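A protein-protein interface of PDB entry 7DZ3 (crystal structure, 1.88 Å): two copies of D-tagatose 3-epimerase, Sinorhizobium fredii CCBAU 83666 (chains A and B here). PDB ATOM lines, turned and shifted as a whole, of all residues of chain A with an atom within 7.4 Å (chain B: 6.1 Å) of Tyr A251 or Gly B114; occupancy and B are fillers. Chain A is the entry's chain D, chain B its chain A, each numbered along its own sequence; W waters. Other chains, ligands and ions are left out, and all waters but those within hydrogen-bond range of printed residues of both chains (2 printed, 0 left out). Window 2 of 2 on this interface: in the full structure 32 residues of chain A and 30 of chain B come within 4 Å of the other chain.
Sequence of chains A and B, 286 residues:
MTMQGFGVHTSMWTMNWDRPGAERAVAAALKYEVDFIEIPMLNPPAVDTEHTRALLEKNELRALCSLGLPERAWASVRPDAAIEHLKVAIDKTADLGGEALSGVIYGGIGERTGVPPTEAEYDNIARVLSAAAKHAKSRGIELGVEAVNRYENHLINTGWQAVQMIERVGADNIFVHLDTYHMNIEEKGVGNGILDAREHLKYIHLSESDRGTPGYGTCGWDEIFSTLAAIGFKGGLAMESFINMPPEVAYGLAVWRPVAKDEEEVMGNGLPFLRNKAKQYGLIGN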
ATOM      1  N   ILE A 109      18.805  -2.520  -3.774  1.00  0.00           N
ATOM      2  CA  ILE A 109      19.777  -3.502  -3.310  1.00  0.00           C
ATOM      3  C   ILE A 109      20.668  -2.790  -2.311  1.00  0.00           C
ATOM      4  O   ILE A 109      21.492  -1.947  -2.684  1.00  0.00           O
ATOM      5  CB  ILE A 109      20.591  -4.095  -4.471  1.00  0.00           C
ATOM      6  CG1 ILE A 109      19.656  -4.872  -5.414  1.00  0.00           C
ATOM      7  CG2 ILE A 109      21.693  -4.992  -3.938  1.00  0.00           C
ATOM      8  CD1 ILE A 109      20.300  -5.243  -6.733  1.00  0.00           C
ATOM      9  N   GLY A 110      20.475  -3.096  -1.047  1.00  0.00           N
ATOM     10  CA  GLY A 110      21.034  -2.333   0.032  1.00  0.00           C
ATOM     11  C   GLY A 110      20.048  -1.448   0.746  1.00  0.00           C
ATOM     12  O   GLY A 110      20.467  -0.639   1.574  1.00  0.00           O
ATOM     13  N   TYR A 151      19.663  -8.570   4.302  1.00  0.00           N
ATOM     14  CA  TYR A 151      20.716  -7.564   4.288  1.00  0.00           C
ATOM     15  C   TYR A 151      20.708  -6.707   3.042  1.00  0.00           C
ATOM     16  O   TYR A 151      21.359  -5.654   3.030  1.00  0.00           O
ATOM     17  CB  TYR A 151      22.089  -8.220   4.372  1.00  0.00           C
ATOM     18  CG  TYR A 151      22.370  -8.979   5.620  1.00  0.00           C
ATOM     19  CD1 TYR A 151      22.570  -8.335   6.826  1.00  0.00           C
ATOM     20  CD2 TYR A 151      22.472 -10.371   5.589  1.00  0.00           C
ATOM     21  CE1 TYR A 151      22.870  -9.036   7.978  1.00  0.00           C
ATOM     22  CE2 TYR A 151      22.757 -11.086   6.717  1.00  0.00           C
ATOM     23  CZ  TYR A 151      22.953 -10.434   7.909  1.00  0.00           C
ATOM     24  OH  TYR A 151      23.251 -11.171   9.016  1.00  0.00           O
ATOM     25  N   MET A 245      31.509  -6.864 -11.148  1.00  0.00           N
ATOM     26  CA  MET A 245      30.512  -6.255 -10.270  1.00  0.00           C
ATOM     27  C   MET A 245      30.047  -4.927 -10.833  1.00  0.00           C
ATOM     28  O   MET A 245      30.841  -3.970 -10.898  1.00  0.00           O
ATOM     29  CB  MET A 245      31.094  -6.100  -8.862  1.00  0.00           C
ATOM     30  CG  MET A 245      30.221  -5.312  -7.870  1.00  0.00           C
ATOM     31  SD  MET A 245      28.575  -6.016  -7.705  1.00  0.00           S
ATOM     32  CE  MET A 245      28.836  -7.417  -6.674  1.00  0.00           C
ATOM     33  N   PRO A 246      28.796  -4.805 -11.261  1.00  0.00           N
ATOM     34  CA  PRO A 246      28.290  -3.493 -11.703  1.00  0.00           C
ATOM     35  C   PRO A 246      28.443  -2.475 -10.592  1.00  0.00           C
ATOM     36  O   PRO A 246      28.153  -2.769  -9.423  1.00  0.00           O
ATOM     37  CB  PRO A 246      26.811  -3.765 -12.028  1.00  0.00           C
ATOM     38  CG  PRO A 246      26.750  -5.255 -12.337  1.00  0.00           C
ATOM     39  CD  PRO A 246      27.784  -5.879 -11.415  1.00  0.00           C
ATOM     40  N   PRO A 247      28.966  -1.292 -10.905  1.00  0.00           N
ATOM     41  CA  PRO A 247      29.278  -0.328  -9.830  1.00  0.00           C
ATOM     42  C   PRO A 247      28.065   0.158  -9.084  1.00  0.00           C
ATOM     43  O   PRO A 247      28.165   0.477  -7.896  1.00  0.00           O
ATOM     44  CB  PRO A 247      29.969   0.833 -10.572  1.00  0.00           C
ATOM     45  CG  PRO A 247      30.481   0.251 -11.827  1.00  0.00           C
ATOM     46  CD  PRO A 247      29.502  -0.859 -12.212  1.00  0.00           C
ATOM     47  N   GLU A 248      26.910   0.239  -9.752  1.00  0.00           N
ATOM     48  CA  GLU A 248      25.711   0.774  -9.119  1.00  0.00           C
ATOM     49  C   GLU A 248      25.221  -0.083  -7.951  1.00  0.00           C
ATOM     50  O   GLU A 248      24.480   0.420  -7.098  1.00  0.00           O
ATOM     51  CB  GLU A 248      24.610   0.905 -10.188  1.00  0.00           C
ATOM     52  CG  GLU A 248      24.974   1.842 -11.367  1.00  0.00           C
ATOM     53  CD  GLU A 248      25.640   1.124 -12.553  1.00  0.00           C
ATOM     54  OE1 GLU A 248      25.997  -0.077 -12.430  1.00  0.00           O
ATOM     55  OE2 GLU A 248      25.798   1.766 -13.626  1.00  0.00           O
ATOM     56  N   VAL A 249      25.628  -1.357  -7.875  1.00  0.00           N
ATOM     57  CA  VAL A 249      25.093  -2.263  -6.867  1.00  0.00           C
ATOM     58  C   VAL A 249      26.186  -2.899  -6.023  1.00  0.00           C
ATOM     59  O   VAL A 249      25.900  -3.757  -5.194  1.00  0.00           O
ATOM     60  CB  VAL A 249      24.209  -3.352  -7.511  1.00  0.00           C
ATOM     61  CG1 VAL A 249      22.853  -2.787  -7.928  1.00  0.00           C
ATOM     62  CG2 VAL A 249      24.912  -3.997  -8.673  1.00  0.00           C
ATOM     63  N   ALA A 250      27.432  -2.489  -6.201  1.00  0.00           N
ATOM     64  CA  ALA A 250      28.510  -3.148  -5.473  1.00  0.00           C
ATOM     65  C   ALA A 250      28.337  -2.965  -3.973  1.00  0.00           C
ATOM     66  O   ALA A 250      28.614  -3.876  -3.190  1.00  0.00           O
ATOM     67  CB  ALA A 250      29.871  -2.602  -5.915  1.00  0.00           C
ATOM     68  N   TYR A 251      27.907  -1.778  -3.551  1.00  0.00           N
ATOM     69  CA  TYR A 251      27.846  -1.523  -2.127  1.00  0.00           C
ATOM     70  C   TYR A 251      26.834  -2.435  -1.456  1.00  0.00           C
ATOM     71  O   TYR A 251      27.066  -2.890  -0.338  1.00  0.00           O
ATOM     72  CB  TYR A 251      27.494  -0.064  -1.873  1.00  0.00           C
ATOM     73  CG  TYR A 251      27.512   0.337  -0.435  1.00  0.00           C
ATOM     74  CD1 TYR A 251      28.691   0.588   0.214  1.00  0.00           C
ATOM     75  CD2 TYR A 251      26.319   0.513   0.265  1.00  0.00           C
ATOM     76  CE1 TYR A 251      28.702   0.983   1.500  1.00  0.00           C
ATOM     77  CE2 TYR A 251      26.331   0.890   1.572  1.00  0.00           C
ATOM     78  CZ  TYR A 251      27.533   1.131   2.183  1.00  0.00           C
ATOM     79  OH  TYR A 251      27.559   1.532   3.497  1.00  0.00           O
ATOM     80  N   GLY A 252      25.708  -2.694  -2.123  1.00  0.00           N
ATOM     81  CA  GLY A 252      24.669  -3.524  -1.530  1.00  0.00           C
ATOM     82  C   GLY A 252      24.909  -5.014  -1.664  1.00  0.00           C
ATOM     83  O   GLY A 252      24.449  -5.792  -0.814  1.00  0.00           O
ATOM     84  N   LEU A 253      25.642  -5.438  -2.698  1.00  0.00           N
ATOM     85  CA  LEU A 253      25.834  -6.874  -2.938  1.00  0.00           C
ATOM     86  C   LEU A 253      26.962  -7.472  -2.110  1.00  0.00           C
ATOM     87  O   LEU A 253      27.013  -8.711  -1.948  1.00  0.00           O
ATOM     88  CB  LEU A 253      26.095  -7.124  -4.424  1.00  0.00           C
ATOM     89  CG  LEU A 253      24.869  -6.954  -5.317  1.00  0.00           C
ATOM     90  CD1 LEU A 253      25.247  -7.039  -6.816  1.00  0.00           C
ATOM     91  CD2 LEU A 253      23.753  -7.984  -4.962  1.00  0.00           C
ATOM     92  N   ALA A 254      27.902  -6.644  -1.659  1.00  0.00           N
ATOM     93  CA  ALA A 254      28.879  -7.018  -0.627  1.00  0.00           C
ATOM     94  C   ALA A 254      29.845  -8.120  -1.058  1.00  0.00           C
ATOM     95  O   ALA A 254      30.141  -9.047  -0.299  1.00  0.00           O
ATOM     96  CB  ALA A 254      28.157  -7.429   0.658  1.00  0.00           C
ATOM     97  N   VAL A 255      30.414  -7.978  -2.256  1.00  0.00           N
ATOM     98  CA  VAL A 255      31.435  -8.900  -2.750  1.00  0.00           C
ATOM     99  C   VAL A 255      32.787  -8.250  -2.474  1.00  0.00           C
ATOM    100  O   VAL A 255      33.232  -7.395  -3.247  1.00  0.00           O
ATOM    101  CB  VAL A 255      31.237  -9.205  -4.235  1.00  0.00           C
ATOM    102  CG1 VAL A 255      32.327 -10.139  -4.753  1.00  0.00           C
ATOM    103  CG2 VAL A 255      29.873  -9.820  -4.462  1.00  0.00           C
ATOM    104  N   TRP A 256      33.436  -8.639  -1.371  1.00  0.00           N
ATOM    105  CA  TRP A 256      34.631  -7.950  -0.897  1.00  0.00           C
ATOM    106  C   TRP A 256      35.896  -8.692  -1.239  1.00  0.00           C
ATOM    107  O   TRP A 256      36.981  -8.257  -0.860  1.00  0.00           O
ATOM    108  CB  TRP A 256      34.615  -7.750   0.620  1.00  0.00           C
ATOM    109  CG  TRP A 256      33.354  -7.183   1.205  1.00  0.00           C
ATOM    110  CD1 TRP A 256      32.715  -7.622   2.337  1.00  0.00           C
ATOM    111  CD2 TRP A 256      32.594  -6.078   0.722  1.00  0.00           C
ATOM    112  NE1 TRP A 256      31.610  -6.870   2.575  1.00  0.00           N
ATOM    113  CE2 TRP A 256      31.509  -5.908   1.605  1.00  0.00           C
ATOM    114  CE3 TRP A 256      32.712  -5.215  -0.382  1.00  0.00           C
ATOM    115  CZ2 TRP A 256      30.550  -4.919   1.428  1.00  0.00           C
ATOM    116  CZ3 TRP A 256      31.754  -4.235  -0.562  1.00  0.00           C
ATOM    117  CH2 TRP A 256      30.695  -4.084   0.345  1.00  0.00           C
ATOM    118  N   GLY B 110      27.834  -3.286  10.827  1.00  0.00           N
ATOM    119  CA  GLY B 110      27.546  -2.117  10.034  1.00  0.00           C
ATOM    120  C   GLY B 110      28.752  -1.471   9.391  1.00  0.00           C
ATOM    121  O   GLY B 110      28.588  -0.458   8.704  1.00  0.00           O
ATOM    122  N   ARG B 112      31.212  -1.067   6.485  1.00  0.00           N
ATOM    123  CA  ARG B 112      31.180  -1.293   5.054  1.00  0.00           C
ATOM    124  C   ARG B 112      31.764  -0.082   4.331  1.00  0.00           C
ATOM    125  O   ARG B 112      31.191   1.006   4.417  1.00  0.00           O
ATOM    126  CB  ARG B 112      29.753  -1.533   4.560  1.00  0.00           C
ATOM    127  CG  ARG B 112      29.732  -2.014   3.113  1.00  0.00           C
ATOM    128  CD  ARG B 112      28.355  -2.442   2.579  1.00  0.00           C
ATOM    129  NE  ARG B 112      27.660  -3.346   3.483  1.00  0.00           N
ATOM    130  CZ  ARG B 112      26.384  -3.699   3.338  1.00  0.00           C
ATOM    131  NH1 ARG B 112      25.707  -3.238   2.304  1.00  0.00           N
ATOM    132  NH2 ARG B 112      25.800  -4.511   4.220  1.00  0.00           N
ATOM    133  N   THR B 113      32.860  -0.255   3.585  1.00  0.00           N
ATOM    134  CA  THR B 113      33.435   0.829   2.795  1.00  0.00           C
ATOM    135  C   THR B 113      32.977   0.820   1.347  1.00  0.00           C
ATOM    136  O   THR B 113      33.056   1.854   0.660  1.00  0.00           O
ATOM    137  CB  THR B 113      34.956   0.731   2.804  1.00  0.00           C
ATOM    138  OG1 THR B 113      35.329  -0.509   2.174  1.00  0.00           O
ATOM    139  CG2 THR B 113      35.487   0.750   4.207  1.00  0.00           C
ATOM    140  N   GLY B 114      32.532  -0.333   0.857  1.00  0.00           N
ATOM    141  CA  GLY B 114      32.136  -0.498  -0.525  1.00  0.00           C
ATOM    142  C   GLY B 114      33.229  -1.061  -1.391  1.00  0.00           C
ATOM    143  O   GLY B 114      33.009  -1.277  -2.590  1.00  0.00           O
ATOM    144  N   VAL B 115      34.399  -1.293  -0.814  1.00  0.00           N
ATOM    145  CA  VAL B 115      35.551  -1.843  -1.527  1.00  0.00           C
ATOM    146  C   VAL B 115      36.176  -2.887  -0.609  1.00  0.00           C
ATOM    147  O   VAL B 115      35.796  -2.974   0.575  1.00  0.00           O
ATOM    148  CB  VAL B 115      36.538  -0.720  -1.889  1.00  0.00           C
ATOM    149  CG1 VAL B 115      35.864   0.322  -2.791  1.00  0.00           C
ATOM    150  CG2 VAL B 115      37.067  -0.072  -0.614  1.00  0.00           C
ATOM    151  N   PRO B 116      37.151  -3.662  -1.084  1.00  0.00           N
ATOM    152  CA  PRO B 116      37.787  -4.680  -0.230  1.00  0.00           C
ATOM    153  C   PRO B 116      38.466  -4.071   0.972  1.00  0.00           C
ATOM    154  O   PRO B 116      38.860  -2.890   0.942  1.00  0.00           O
ATOM    155  CB  PRO B 116      38.826  -5.351  -1.148  1.00  0.00           C
ATOM    156  CG  PRO B 116      38.296  -5.139  -2.521  1.00  0.00           C
ATOM    157  CD  PRO B 116      37.545  -3.810  -2.500  1.00  0.00           C
ATOM    158  N   HIS B 154      33.094  -5.956   6.581  1.00  0.00           N
ATOM    159  CA  HIS B 154      33.812  -6.301   5.358  1.00  0.00           C
ATOM    160  C   HIS B 154      35.200  -6.818   5.639  1.00  0.00           C
ATOM    161  O   HIS B 154      35.938  -7.085   4.706  1.00  0.00           O
ATOM    162  CB  HIS B 154      33.883  -5.089   4.425  1.00  0.00           C
ATOM    163  CG  HIS B 154      34.702  -3.975   4.979  1.00  0.00           C
ATOM    164  ND1 HIS B 154      34.340  -3.302   6.130  1.00  0.00           N
ATOM    165  CD2 HIS B 154      35.887  -3.447   4.577  1.00  0.00           C
ATOM    166  CE1 HIS B 154      35.256  -2.385   6.401  1.00  0.00           C
ATOM    167  NE2 HIS B 154      36.210  -2.464   5.487  1.00  0.00           N
HETATM  168  O   HOH W   1      23.009  -4.528   4.627  1.00  0.00           O
HETATM  169  O   HOH W   2      23.468  -4.672   1.469  1.00  0.00           O
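Of the 7 printed residues of chain B, 5 touch a printed residue of chain A. Hydrophobic or aromatic side chains of chain A that line the printed part of chain B: Tyr A251 and Trp A256. Among the printed residues, 8 pairs touch across the chains. Among the printed residues, no Asp or Glu carboxylate lies within 4 Å of a Lys or Arg side-chain nitrogen of the other chain.
1 position is printed for both chains.
Among the printed residues, merely in contact across the chains: Tyr A251 with Gly B114 (3.7 Å), Gly A252 with Arg B112 (3.98 Å), Trp A256 with Arg B112 (3.5 Å), Trp A256 with Gly B114 (3.6 Å), Trp A256 with Val B115 (3.9 Å), Trp A256 with Pro B116 (3.5 Å) and Trp A256 with His B154 (3.4 Å).
Tyr A251 touches just these residues of chain B: Arg B112 (3.0 Å) and Gly B114 (3.7 Å). Printed residues of chain B within 4 Å of Gly A252: Arg B112. Of the printed residues of chain B, Trp A256 touches Arg B112, Gly B114, Val B115, Pro B116 and His B154. Of the printed residues of chain A, Gly B114 touches Tyr A251 (3.7 Å) and Trp A256 (3.6 Å). The nearest printed residue of chain B that does not touch Trp A256 is Thr B113 (5.5 Å).
The guanidinium group (NH1) of Arg B112 sits at hydrogen-bond distance from the backbone carbonyl oxygen (O) of Tyr A251.
Water W1 bridges O of Tyr A151 and NH2 of Arg B112. Water W2 lies within hydrogen-bond range of the backbone carbonyl oxygen of Gly A252, the guanidinium group of Arg B112 and the backbone carbonyl oxygen of Tyr A151.
OG1 of Thr B113 is in hydrogen-bond range of O of Val B115.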
